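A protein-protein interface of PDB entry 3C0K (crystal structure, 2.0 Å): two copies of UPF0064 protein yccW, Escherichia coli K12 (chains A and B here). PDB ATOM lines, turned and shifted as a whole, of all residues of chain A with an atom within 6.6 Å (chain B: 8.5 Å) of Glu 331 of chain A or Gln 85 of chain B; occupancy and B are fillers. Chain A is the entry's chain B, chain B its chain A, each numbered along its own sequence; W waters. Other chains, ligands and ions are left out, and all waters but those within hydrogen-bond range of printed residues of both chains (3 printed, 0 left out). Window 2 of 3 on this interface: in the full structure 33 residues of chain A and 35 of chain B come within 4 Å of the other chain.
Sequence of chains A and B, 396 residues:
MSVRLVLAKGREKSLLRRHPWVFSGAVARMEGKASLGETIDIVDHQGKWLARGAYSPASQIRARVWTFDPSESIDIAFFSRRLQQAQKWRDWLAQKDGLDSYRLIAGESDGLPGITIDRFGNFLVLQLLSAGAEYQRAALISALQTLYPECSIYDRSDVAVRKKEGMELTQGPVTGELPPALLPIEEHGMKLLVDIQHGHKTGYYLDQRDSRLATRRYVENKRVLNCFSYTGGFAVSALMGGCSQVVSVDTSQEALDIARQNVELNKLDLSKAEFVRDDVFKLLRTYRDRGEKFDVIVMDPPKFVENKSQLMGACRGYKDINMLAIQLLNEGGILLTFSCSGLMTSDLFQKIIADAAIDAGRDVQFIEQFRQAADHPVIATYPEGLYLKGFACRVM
The backbone NH (N) of Gly 332 of chain A is in hydrogen-bond range of the backbone carbonyl oxygen (O) of Val 395 of chain A (2.9 Å).
The side-chain amino group of Lys 88 of chain B lies close to the guanidinium group of Arg 394 of chain A, at 3.4 Å.
No position is printed for both chains.
NE2 of Gln 85 of chain B touches OE1 of Glu 331 of chain A (3.9 Å).
Gly 332 of chain A touches Lys 88 of chain B (CA to CE, 3.6 Å).
Trp 89 of chain B touches Arg 394 of chain A.
Printed residues of chain A that touch a printed residue of chain B: Glu 331, Gly 332 and Arg 394.
Hydrophobic or aromatic side chains of chain B within 4 Å of the printed part of chain A: Trp 89.
Along chain B the printed residues that touch a printed residue of chain A span positions 85 to 89.
Water W2 bridges the chain-end carboxylate (OXT) of Met 396 of chain A (2.5 Å) and the side-chain amide oxygen (OE1) of Gln 85 of chain B (3.3 Å).
Water W1 lies within hydrogen-bond range of the side-chain amino group (NZ) of Lys 88 of chain B (2.6 Å), the backbone carbonyl oxygen (O) of Gly 332 of chain A (2.6 Å) and the guanidinium group (NE) of Arg 394 of chain A (2.8 Å).
Water W3 lies within hydrogen-bond range of the backbone carbonyl oxygen of Gln 85 of chain B and the guanidinium group of Arg 394 of chain A.
Gln 85 of chain B touches one residue of chain A.
Gly 332 of chain A touches one residue of chain B.
Of the printed residues of chain A, Lys 88 of chain B touches Gly 332 (3.6 Å) and Arg 394 (2.9 Å).
Of the printed residues of chain A, Trp 89 of chain B touches Arg 394.
Printed residues of chain B within 4 Å of Arg 394 of chain A: Lys 88 and Trp 89.
The nearest residue of chain A that does not touch Gln 85 of chain B is Arg 394 of chain A (4.2 Å).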
ATOM      1  N   LYS A 293      13.885 -15.660 -10.663  1.00  0.00           N
ATOM      2  CA  LYS A 293      13.567 -15.179 -11.999  1.00  0.00           C
ATOM      3  C   LYS A 293      14.584 -14.176 -12.518  1.00  0.00           C
ATOM      4  O   LYS A 293      15.112 -13.366 -11.758  1.00  0.00           O
ATOM      5  CB  LYS A 293      12.173 -14.545 -12.008  1.00  0.00           C
ATOM      6  CG  LYS A 293      11.031 -15.543 -11.914  1.00  0.00           C
ATOM      7  CD  LYS A 293      10.938 -16.410 -13.170  1.00  0.00           C
ATOM      8  CE  LYS A 293       9.731 -17.324 -13.096  1.00  0.00           C
ATOM      9  NZ  LYS A 293       9.534 -18.085 -14.358  1.00  0.00           N
ATOM     10  N   PHE A 294      14.852 -14.243 -13.820  1.00  0.00           N
ATOM     11  CA  PHE A 294      15.793 -13.340 -14.481  1.00  0.00           C
ATOM     12  C   PHE A 294      15.161 -12.785 -15.756  1.00  0.00           C
ATOM     13  O   PHE A 294      14.219 -13.373 -16.293  1.00  0.00           O
ATOM     14  CB  PHE A 294      17.086 -14.090 -14.828  1.00  0.00           C
ATOM     15  CG  PHE A 294      17.901 -14.467 -13.630  1.00  0.00           C
ATOM     16  CD1 PHE A 294      18.785 -13.555 -13.063  1.00  0.00           C
ATOM     17  CD2 PHE A 294      17.770 -15.727 -13.050  1.00  0.00           C
ATOM     18  CE1 PHE A 294      19.532 -13.889 -11.935  1.00  0.00           C
ATOM     19  CE2 PHE A 294      18.512 -16.072 -11.919  1.00  0.00           C
ATOM     20  CZ  PHE A 294      19.394 -15.152 -11.362  1.00  0.00           C
ATOM     21  N   ASP A 295      15.682 -11.659 -16.235  1.00  0.00           N
ATOM     22  CA  ASP A 295      15.177 -11.029 -17.455  1.00  0.00           C
ATOM     23  C   ASP A 295      16.015 -11.464 -18.651  1.00  0.00           C
ATOM     24  O   ASP A 295      15.511 -11.574 -19.771  1.00  0.00           O
ATOM     25  CB  ASP A 295      15.239  -9.503 -17.329  1.00  0.00           C
ATOM     26  CG  ASP A 295      14.483  -8.989 -16.121  1.00  0.00           C
ATOM     27  OD1 ASP A 295      13.288  -9.335 -15.983  1.00  0.00           O
ATOM     28  OD2 ASP A 295      15.077  -8.240 -15.315  1.00  0.00           O
ATOM     29  N   LEU A 329      13.135 -17.691 -16.601  1.00  0.00           N
ATOM     30  CA  LEU A 329      12.852 -16.416 -17.248  1.00  0.00           C
ATOM     31  C   LEU A 329      11.461 -15.858 -16.975  1.00  0.00           C
ATOM     32  O   LEU A 329      10.487 -16.602 -16.889  1.00  0.00           O
ATOM     33  CB  LEU A 329      13.044 -16.549 -18.766  1.00  0.00           C
ATOM     34  CG  LEU A 329      14.485 -16.608 -19.277  1.00  0.00           C
ATOM     35  CD1 LEU A 329      14.489 -16.875 -20.764  1.00  0.00           C
ATOM     36  CD2 LEU A 329      15.184 -15.286 -18.979  1.00  0.00           C
ATOM     37  N   ASN A 330      11.392 -14.537 -16.830  1.00  0.00           N
ATOM     38  CA  ASN A 330      10.124 -13.837 -16.623  1.00  0.00           C
ATOM     39  C   ASN A 330       9.468 -13.791 -18.010  1.00  0.00           C
ATOM     40  O   ASN A 330      10.082 -14.179 -19.005  1.00  0.00           O
ATOM     41  CB  ASN A 330      10.361 -12.386 -16.158  1.00  0.00           C
ATOM     42  CG  ASN A 330      10.811 -12.280 -14.706  1.00  0.00           C
ATOM     43  OD1 ASN A 330      10.173 -12.820 -13.803  1.00  0.00           O
ATOM     44  ND2 ASN A 330      11.908 -11.556 -14.474  1.00  0.00           N
ATOM     45  N   GLU A 331       8.227 -13.327 -18.087  1.00  0.00           N
ATOM     46  CA  GLU A 331       7.585 -13.219 -19.391  1.00  0.00           C
ATOM     47  C   GLU A 331       8.341 -12.093 -20.093  1.00  0.00           C
ATOM     48  O   GLU A 331       8.577 -11.046 -19.502  1.00  0.00           O
ATOM     49  CB  GLU A 331       6.104 -12.854 -19.245  1.00  0.00           C
ATOM     50  CG  GLU A 331       5.449 -12.436 -20.559  1.00  0.00           C
ATOM     51  CD  GLU A 331       3.934 -12.321 -20.464  1.00  0.00           C
ATOM     52  OE1 GLU A 331       3.321 -11.777 -21.409  1.00  0.00           O
ATOM     53  OE2 GLU A 331       3.359 -12.785 -19.453  1.00  0.00           O
ATOM     54  N   GLY A 332       8.735 -12.313 -21.341  1.00  0.00           N
ATOM     55  CA  GLY A 332       9.481 -11.293 -22.055  1.00  0.00           C
ATOM     56  C   GLY A 332      10.970 -11.454 -21.794  1.00  0.00           C
ATOM     57  O   GLY A 332      11.790 -10.689 -22.294  1.00  0.00           O
ATOM     58  N   GLY A 333      11.317 -12.459 -20.997  1.00  0.00           N
ATOM     59  CA  GLY A 333      12.708 -12.717 -20.700  1.00  0.00           C
ATOM     60  C   GLY A 333      13.411 -13.155 -21.968  1.00  0.00           C
ATOM     61  O   GLY A 333      12.793 -13.726 -22.871  1.00  0.00           O
ATOM     62  N   ARG A 362       6.356 -23.418 -22.033  1.00  0.00           N
ATOM     63  CA  ARG A 362       6.355 -22.033 -22.487  1.00  0.00           C
ATOM     64  C   ARG A 362       6.850 -21.937 -23.926  1.00  0.00           C
ATOM     65  O   ARG A 362       7.760 -22.661 -24.325  1.00  0.00           O
ATOM     66  CB  ARG A 362       7.252 -21.192 -21.573  1.00  0.00           C
ATOM     67  CG  ARG A 362       6.868 -21.281 -20.106  1.00  0.00           C
ATOM     68  CD  ARG A 362       7.943 -20.695 -19.215  1.00  0.00           C
ATOM     69  NE  ARG A 362       7.960 -19.234 -19.230  1.00  0.00           N
ATOM     70  CZ  ARG A 362       7.296 -18.468 -18.372  1.00  0.00           C
ATOM     71  NH1 ARG A 362       6.553 -19.018 -17.421  1.00  0.00           N
ATOM     72  NH2 ARG A 362       7.391 -17.148 -18.452  1.00  0.00           N
ATOM     73  N   ARG A 394      13.041 -15.300 -27.016  1.00  0.00           N
ATOM     74  CA  ARG A 394      12.176 -14.554 -26.122  1.00  0.00           C
ATOM     75  C   ARG A 394      11.002 -15.404 -25.645  1.00  0.00           C
ATOM     76  O   ARG A 394      10.281 -16.002 -26.450  1.00  0.00           O
ATOM     77  CB  ARG A 394      11.673 -13.301 -26.842  1.00  0.00           C
ATOM     78  CG  ARG A 394      10.784 -12.423 -26.010  1.00  0.00           C
ATOM     79  CD  ARG A 394      10.439 -11.132 -26.749  1.00  0.00           C
ATOM     80  NE  ARG A 394       9.436 -10.399 -25.996  1.00  0.00           N
ATOM     81  CZ  ARG A 394       8.147 -10.707 -25.993  1.00  0.00           C
ATOM     82  NH1 ARG A 394       7.709 -11.726 -26.724  1.00  0.00           N
ATOM     83  NH2 ARG A 394       7.305 -10.029 -25.230  1.00  0.00           N
ATOM     84  N   VAL A 395      10.820 -15.461 -24.328  1.00  0.00           N
ATOM     85  CA  VAL A 395       9.734 -16.227 -23.725  1.00  0.00           C
ATOM     86  C   VAL A 395       8.439 -15.441 -23.890  1.00  0.00           C
ATOM     87  O   VAL A 395       8.357 -14.281 -23.491  1.00  0.00           O
ATOM     88  CB  VAL A 395       9.994 -16.469 -22.224  1.00  0.00           C
ATOM     89  CG1 VAL A 395       8.835 -17.245 -21.610  1.00  0.00           C
ATOM     90  CG2 VAL A 395      11.300 -17.232 -22.042  1.00  0.00           C
ATOM     91  N   MET A 396       7.425 -16.066 -24.479  1.00  0.00           N
ATOM     92  CA  MET A 396       6.160 -15.379 -24.700  1.00  0.00           C
ATOM     93  C   MET A 396       5.291 -15.360 -23.444  1.00  0.00           C
ATOM     94  O   MET A 396       5.398 -16.303 -22.636  1.00  0.00           O
ATOM     95  OXT MET A 396       4.506 -14.400 -23.286  1.00  0.00           O
ATOM     96  CB  MET A 396       5.406 -16.041 -25.860  1.00  0.00           C
ATOM     97  CG  MET A 396       6.154 -15.980 -27.186  1.00  0.00           C
ATOM     98  SD  MET A 396       5.308 -16.834 -28.553  1.00  0.00           S
ATOM     99  CE  MET A 396       4.075 -15.603 -28.974  1.00  0.00           C
ATOM    100  N   GLU B  72     -10.303 -21.139 -23.854  1.00  0.00           N
ATOM    101  CA  GLU B  72     -10.166 -19.879 -24.560  1.00  0.00           C
ATOM    102  C   GLU B  72     -11.044 -19.770 -25.797  1.00  0.00           C
ATOM    103  O   GLU B  72     -10.846 -20.492 -26.776  1.00  0.00           O
ATOM    104  CB  GLU B  72      -8.704 -19.666 -24.940  1.00  0.00           C
ATOM    105  CG  GLU B  72      -8.416 -18.326 -25.567  1.00  0.00           C
ATOM    106  CD  GLU B  72      -6.949 -17.976 -25.492  1.00  0.00           C
ATOM    107  OE1 GLU B  72      -6.115 -18.845 -25.811  1.00  0.00           O
ATOM    108  OE2 GLU B  72      -6.628 -16.829 -25.122  1.00  0.00           O
ATOM    109  N   ALA B  77     -11.914 -10.298 -27.041  1.00  0.00           N
ATOM    110  CA  ALA B  77     -10.959 -10.392 -25.943  1.00  0.00           C
ATOM    111  C   ALA B  77      -9.713 -11.192 -26.311  1.00  0.00           C
ATOM    112  O   ALA B  77      -8.613 -10.877 -25.858  1.00  0.00           O
ATOM    113  CB  ALA B  77     -11.627 -11.011 -24.721  1.00  0.00           C
ATOM    114  N   PHE B  78      -9.901 -12.237 -27.111  1.00  0.00           N
ATOM    115  CA  PHE B  78      -8.809 -13.099 -27.558  1.00  0.00           C
ATOM    116  C   PHE B  78      -7.786 -12.272 -28.334  1.00  0.00           C
ATOM    117  O   PHE B  78      -6.585 -12.333 -28.064  1.00  0.00           O
ATOM    118  CB  PHE B  78      -9.359 -14.217 -28.453  1.00  0.00           C
ATOM    119  CG  PHE B  78      -8.295 -15.000 -29.186  1.00  0.00           C
ATOM    120  CD1 PHE B  78      -7.490 -15.914 -28.510  1.00  0.00           C
ATOM    121  CD2 PHE B  78      -8.103 -14.819 -30.556  1.00  0.00           C
ATOM    122  CE1 PHE B  78      -6.508 -16.640 -29.188  1.00  0.00           C
ATOM    123  CE2 PHE B  78      -7.121 -15.540 -31.248  1.00  0.00           C
ATOM    124  CZ  PHE B  78      -6.322 -16.454 -30.561  1.00  0.00           C
ATOM    125  N   PHE B  79      -8.274 -11.493 -29.296  1.00  0.00           N
ATOM    126  CA  PHE B  79      -7.407 -10.663 -30.114  1.00  0.00           C
ATOM    127  C   PHE B  79      -6.806  -9.531 -29.308  1.00  0.00           C
ATOM    128  O   PHE B  79      -5.664  -9.143 -29.537  1.00  0.00           O
ATOM    129  CB  PHE B  79      -8.185 -10.112 -31.309  1.00  0.00           C
ATOM    130  CG  PHE B  79      -8.598 -11.173 -32.287  1.00  0.00           C
ATOM    131  CD1 PHE B  79      -7.654 -11.766 -33.125  1.00  0.00           C
ATOM    132  CD2 PHE B  79      -9.914 -11.617 -32.337  1.00  0.00           C
ATOM    133  CE1 PHE B  79      -8.018 -12.792 -33.997  1.00  0.00           C
ATOM    134  CE2 PHE B  79     -10.289 -12.643 -33.201  1.00  0.00           C
ATOM    135  CZ  PHE B  79      -9.341 -13.231 -34.031  1.00  0.00           C
ATOM    136  N   SER B  80      -7.578  -9.008 -28.361  1.00  0.00           N
ATOM    137  CA  SER B  80      -7.104  -7.927 -27.512  1.00  0.00           C
ATOM    138  C   SER B  80      -5.889  -8.397 -26.697  1.00  0.00           C
ATOM    139  O   SER B  80      -4.881  -7.699 -26.621  1.00  0.00           O
ATOM    140  CB  SER B  80      -8.230  -7.468 -26.582  1.00  0.00           C
ATOM    141  OG  SER B  80      -7.800  -6.390 -25.770  1.00  0.00           O
ATOM    142  N   ARG B  81      -5.985  -9.583 -26.101  1.00  0.00           N
ATOM    143  CA  ARG B  81      -4.881 -10.126 -25.313  1.00  0.00           C
ATOM    144  C   ARG B  81      -3.655 -10.409 -26.177  1.00  0.00           C
ATOM    145  O   ARG B  81      -2.524 -10.162 -25.764  1.00  0.00           O
ATOM    146  CB  ARG B  81      -5.302 -11.415 -24.599  1.00  0.00           C
ATOM    147  CG  ARG B  81      -6.211 -11.202 -23.390  1.00  0.00           C
ATOM    148  CD  ARG B  81      -6.308 -12.469 -22.547  1.00  0.00           C
ATOM    149  NE  ARG B  81      -6.970 -13.570 -23.244  1.00  0.00           N
ATOM    150  CZ  ARG B  81      -8.285 -13.655 -23.436  1.00  0.00           C
ATOM    151  NH1 ARG B  81      -9.088 -12.702 -22.985  1.00  0.00           N
ATOM    152  NH2 ARG B  81      -8.799 -14.702 -24.065  1.00  0.00           N
ATOM    153  N   ARG B  82      -3.884 -10.933 -27.375  1.00  0.00           N
ATOM    154  CA  ARG B  82      -2.790 -11.248 -28.294  1.00  0.00           C
ATOM    155  C   ARG B  82      -2.088  -9.977 -28.748  1.00  0.00           C
ATOM    156  O   ARG B  82      -0.862  -9.936 -28.826  1.00  0.00           O
ATOM    157  CB  ARG B  82      -3.324 -12.005 -29.512  1.00  0.00           C
ATOM    158  CG  ARG B  82      -3.715 -13.445 -29.231  1.00  0.00           C
ATOM    159  CD  ARG B  82      -2.474 -14.316 -29.134  1.00  0.00           C
ATOM    160  NE  ARG B  82      -2.771 -15.723 -29.387  1.00  0.00           N
ATOM    161  CZ  ARG B  82      -3.165 -16.585 -28.457  1.00  0.00           C
ATOM    162  NH1 ARG B  82      -3.308 -16.184 -27.203  1.00  0.00           N
ATOM    163  NH2 ARG B  82      -3.407 -17.849 -28.785  1.00  0.00           N
ATOM    164  N   LEU B  83      -2.872  -8.949 -29.062  1.00  0.00           N
ATOM    165  CA  LEU B  83      -2.325  -7.666 -29.487  1.00  0.00           C
ATOM    166  C   LEU B  83      -1.508  -7.019 -28.370  1.00  0.00           C
ATOM    167  O   LEU B  83      -0.449  -6.444 -28.616  1.00  0.00           O
ATOM    168  CB  LEU B  83      -3.460  -6.718 -29.911  1.00  0.00           C
ATOM    169  CG  LEU B  83      -4.131  -7.070 -31.240  1.00  0.00           C
ATOM    170  CD1 LEU B  83      -5.478  -6.355 -31.372  1.00  0.00           C
ATOM    171  CD2 LEU B  83      -3.188  -6.696 -32.378  1.00  0.00           C
ATOM    172  N   GLN B  84      -2.008  -7.100 -27.142  1.00  0.00           N
ATOM    173  CA  GLN B  84      -1.302  -6.512 -26.003  1.00  0.00           C
ATOM    174  C   GLN B  84       0.007  -7.247 -25.723  1.00  0.00           C
ATOM    175  O   GLN B  84       1.023  -6.624 -25.417  1.00  0.00           O
ATOM    176  CB  GLN B  84      -2.188  -6.535 -24.756  1.00  0.00           C
ATOM    177  CG  GLN B  84      -3.189  -5.387 -24.691  1.00  0.00           C
ATOM    178  CD  GLN B  84      -4.136  -5.504 -23.515  1.00  0.00           C
ATOM    179  OE1 GLN B  84      -5.191  -6.129 -23.611  1.00  0.00           O
ATOM    180  NE2 GLN B  84      -3.755  -4.914 -22.389  1.00  0.00           N
ATOM    181  N   GLN B  85      -0.012  -8.571 -25.827  1.00  0.00           N
ATOM    182  CA  GLN B  85       1.199  -9.339 -25.583  1.00  0.00           C
ATOM    183  C   GLN B  85       2.249  -9.018 -26.648  1.00  0.00           C
ATOM    184  O   GLN B  85       3.435  -8.888 -26.340  1.00  0.00           O
ATOM    185  CB  GLN B  85       0.872 -10.835 -25.540  1.00  0.00           C
ATOM    186  CG  GLN B  85      -0.024 -11.180 -24.356  1.00  0.00           C
ATOM    187  CD  GLN B  85      -0.231 -12.667 -24.151  1.00  0.00           C
ATOM    188  OE1 GLN B  85      -0.585 -13.394 -25.081  1.00  0.00           O
ATOM    189  NE2 GLN B  85      -0.024 -13.127 -22.919  1.00  0.00           N
ATOM    190  N   ALA B  86       1.807  -8.864 -27.896  1.00  0.00           N
ATOM    191  CA  ALA B  86       2.718  -8.531 -28.990  1.00  0.00           C
ATOM    192  C   ALA B  86       3.252  -7.103 -28.827  1.00  0.00           C
ATOM    193  O   ALA B  86       4.432  -6.842 -29.057  1.00  0.00           O
ATOM    194  CB  ALA B  86       2.004  -8.669 -30.337  1.00  0.00           C
ATOM    195  N   GLN B  87       2.378  -6.186 -28.421  1.00  0.00           N
ATOM    196  CA  GLN B  87       2.759  -4.788 -28.240  1.00  0.00           C
ATOM    197  C   GLN B  87       3.865  -4.633 -27.205  1.00  0.00           C
ATOM    198  O   GLN B  87       4.700  -3.734 -27.308  1.00  0.00           O
ATOM    199  CB  GLN B  87       1.549  -3.954 -27.805  1.00  0.00           C
ATOM    200  CG  GLN B  87       1.820  -2.453 -27.746  1.00  0.00           C
ATOM    201  CD  GLN B  87       2.061  -1.851 -29.119  1.00  0.00           C
ATOM    202  OE1 GLN B  87       1.200  -1.919 -29.996  1.00  0.00           O
ATOM    203  NE2 GLN B  87       3.230  -1.256 -29.312  1.00  0.00           N
ATOM    204  N   LYS B  88       3.866  -5.505 -26.203  1.00  0.00           N
ATOM    205  CA  LYS B  88       4.880  -5.443 -25.161  1.00  0.00           C
ATOM    206  C   LYS B  88       6.278  -5.551 -25.758  1.00  0.00           C
ATOM    207  O   LYS B  88       7.177  -4.802 -25.380  1.00  0.00           O
ATOM    208  CB  LYS B  88       4.660  -6.557 -24.136  1.00  0.00           C
ATOM    209  CG  LYS B  88       5.817  -6.718 -23.156  1.00  0.00           C
ATOM    210  CD  LYS B  88       6.474  -8.087 -23.312  1.00  0.00           C
ATOM    211  CE  LYS B  88       7.928  -8.099 -22.843  1.00  0.00           C
ATOM    212  NZ  LYS B  88       8.843  -7.386 -23.777  1.00  0.00           N
ATOM    213  N   TRP B  89       6.457  -6.476 -26.700  1.00  0.00           N
ATOM    214  CA  TRP B  89       7.754  -6.676 -27.348  1.00  0.00           C
ATOM    215  C   TRP B  89       8.142  -5.482 -28.216  1.00  0.00           C
ATOM    216  O   TRP B  89       9.278  -5.016 -28.159  1.00  0.00           O
ATOM    217  CB  TRP B  89       7.730  -7.948 -28.212  1.00  0.00           C
ATOM    218  CG  TRP B  89       8.992  -8.199 -29.035  1.00  0.00           C
ATOM    219  CD1 TRP B  89       9.046  -8.568 -30.353  1.00  0.00           C
ATOM    220  CD2 TRP B  89      10.356  -8.162 -28.577  1.00  0.00           C
ATOM    221  NE1 TRP B  89      10.350  -8.767 -30.740  1.00  0.00           N
ATOM    222  CE2 TRP B  89      11.174  -8.527 -29.672  1.00  0.00           C
ATOM    223  CE3 TRP B  89      10.963  -7.861 -27.349  1.00  0.00           C
ATOM    224  CZ2 TRP B  89      12.573  -8.600 -29.576  1.00  0.00           C
ATOM    225  CZ3 TRP B  89      12.360  -7.933 -27.254  1.00  0.00           C
ATOM    226  CH2 TRP B  89      13.145  -8.300 -28.362  1.00  0.00           C
ATOM    227  N   ARG B  90       7.200  -4.985 -29.017  1.00  0.00           N
ATOM    228  CA  ARG B  90       7.475  -3.855 -29.902  1.00  0.00           C
ATOM    229  C   ARG B  90       7.722  -2.543 -29.177  1.00  0.00           C
ATOM    230  O   ARG B  90       8.401  -1.666 -29.709  1.00  0.00           O
ATOM    231  CB  ARG B  90       6.351  -3.682 -30.928  1.00  0.00           C
ATOM    232  CG  ARG B  90       6.451  -4.646 -32.105  1.00  0.00           C
ATOM    233  CD  ARG B  90       6.261  -6.092 -31.680  1.00  0.00           C
ATOM    234  NE  ARG B  90       6.277  -7.006 -32.818  1.00  0.00           N
ATOM    235  CZ  ARG B  90       5.873  -8.272 -32.768  1.00  0.00           C
ATOM    236  NH1 ARG B  90       5.414  -8.782 -31.635  1.00  0.00           N
ATOM    237  NH2 ARG B  90       5.924  -9.030 -33.855  1.00  0.00           N
ATOM    238  N   ASP B  91       7.174  -2.393 -27.976  1.00  0.00           N
ATOM    239  CA  ASP B  91       7.422  -1.178 -27.212  1.00  0.00           C
ATOM    240  C   ASP B  91       8.902  -1.157 -26.847  1.00  0.00           C
ATOM    241  O   ASP B  91       9.558  -0.115 -26.910  1.00  0.00           O
ATOM    242  CB  ASP B  91       6.573  -1.136 -25.934  1.00  0.00           C
ATOM    243  CG  ASP B  91       5.124  -0.775 -26.205  1.00  0.00           C
ATOM    244  OD1 ASP B  91       4.859  -0.086 -27.215  1.00  0.00           O
ATOM    245  OD2 ASP B  91       4.252  -1.164 -25.404  1.00  0.00           O
ATOM    246  N   LEU B 104       3.676  -5.270 -35.891  1.00  0.00           N
ATOM    247  CA  LEU B 104       3.068  -5.539 -34.591  1.00  0.00           C
ATOM    248  C   LEU B 104       2.737  -7.013 -34.435  1.00  0.00           C
ATOM    249  O   LEU B 104       3.092  -7.646 -33.436  1.00  0.00           O
ATOM    250  CB  LEU B 104       1.798  -4.696 -34.412  1.00  0.00           C
ATOM    251  CG  LEU B 104       1.012  -4.859 -33.107  1.00  0.00           C
ATOM    252  CD1 LEU B 104       1.950  -4.757 -31.900  1.00  0.00           C
ATOM    253  CD2 LEU B 104      -0.063  -3.786 -33.049  1.00  0.00           C
ATOM    254  N   ASP B 110       3.037 -14.707 -33.462  1.00  0.00           N
ATOM    255  CA  ASP B 110       2.460 -13.898 -32.399  1.00  0.00           C
ATOM    256  C   ASP B 110       1.086 -14.478 -32.029  1.00  0.00           C
ATOM    257  O   ASP B 110       0.183 -13.767 -31.592  1.00  0.00           O
ATOM    258  CB  ASP B 110       2.342 -12.431 -32.836  1.00  0.00           C
ATOM    259  CG  ASP B 110       3.690 -11.705 -32.823  1.00  0.00           C
ATOM    260  OD1 ASP B 110       4.326 -11.640 -31.743  1.00  0.00           O
ATOM    261  OD2 ASP B 110       4.118 -11.204 -33.885  1.00  0.00           O
ATOM    262  N   GLY B 111       0.946 -15.786 -32.217  1.00  0.00           N
ATOM    263  CA  GLY B 111      -0.298 -16.470 -31.895  1.00  0.00           C
ATOM    264  C   GLY B 111      -1.537 -16.125 -32.714  1.00  0.00           C
ATOM    265  O   GLY B 111      -2.643 -16.464 -32.305  1.00  0.00           O
ATOM    266  N   LEU B 147      -7.864  -0.835 -28.412  1.00  0.00           N
ATOM    267  CA  LEU B 147      -6.492  -0.662 -27.930  1.00  0.00           C
ATOM    268  C   LEU B 147      -5.747   0.526 -28.540  1.00  0.00           C
ATOM    269  O   LEU B 147      -4.871   1.102 -27.901  1.00  0.00           O
ATOM    270  CB  LEU B 147      -5.688  -1.950 -28.173  1.00  0.00           C
ATOM    271  CG  LEU B 147      -6.110  -3.177 -27.357  1.00  0.00           C
ATOM    272  CD1 LEU B 147      -5.353  -4.411 -27.828  1.00  0.00           C
ATOM    273  CD2 LEU B 147      -5.845  -2.916 -25.883  1.00  0.00           C
ATOM    274  N   TYR B 148      -6.103   0.896 -29.768  1.00  0.00           N
ATOM    275  CA  TYR B 148      -5.455   2.005 -30.475  1.00  0.00           C
ATOM    276  C   TYR B 148      -6.524   2.946 -31.038  1.00  0.00           C
ATOM    277  O   TYR B 148      -6.616   3.144 -32.246  1.00  0.00           O
ATOM    278  CB  TYR B 148      -4.590   1.449 -31.619  1.00  0.00           C
ATOM    279  CG  TYR B 148      -3.653   0.341 -31.180  1.00  0.00           C
ATOM    280  CD1 TYR B 148      -2.443   0.635 -30.551  1.00  0.00           C
ATOM    281  CD2 TYR B 148      -4.007  -1.004 -31.334  1.00  0.00           C
ATOM    282  CE1 TYR B 148      -1.609  -0.378 -30.081  1.00  0.00           C
ATOM    283  CE2 TYR B 148      -3.180  -2.030 -30.864  1.00  0.00           C
ATOM    284  CZ  TYR B 148      -1.982  -1.705 -30.235  1.00  0.00           C
ATOM    285  OH  TYR B 148      -1.176  -2.697 -29.730  1.00  0.00           O
HETATM  286  O   HOH W   1      10.920  -8.964 -24.089  1.00  0.00           O
HETATM  287  O   HOH W   2       2.595 -14.080 -24.938  1.00  0.00           O
HETATM  288  O   HOH W   3       4.669 -10.439 -24.472  1.00  0.00           O
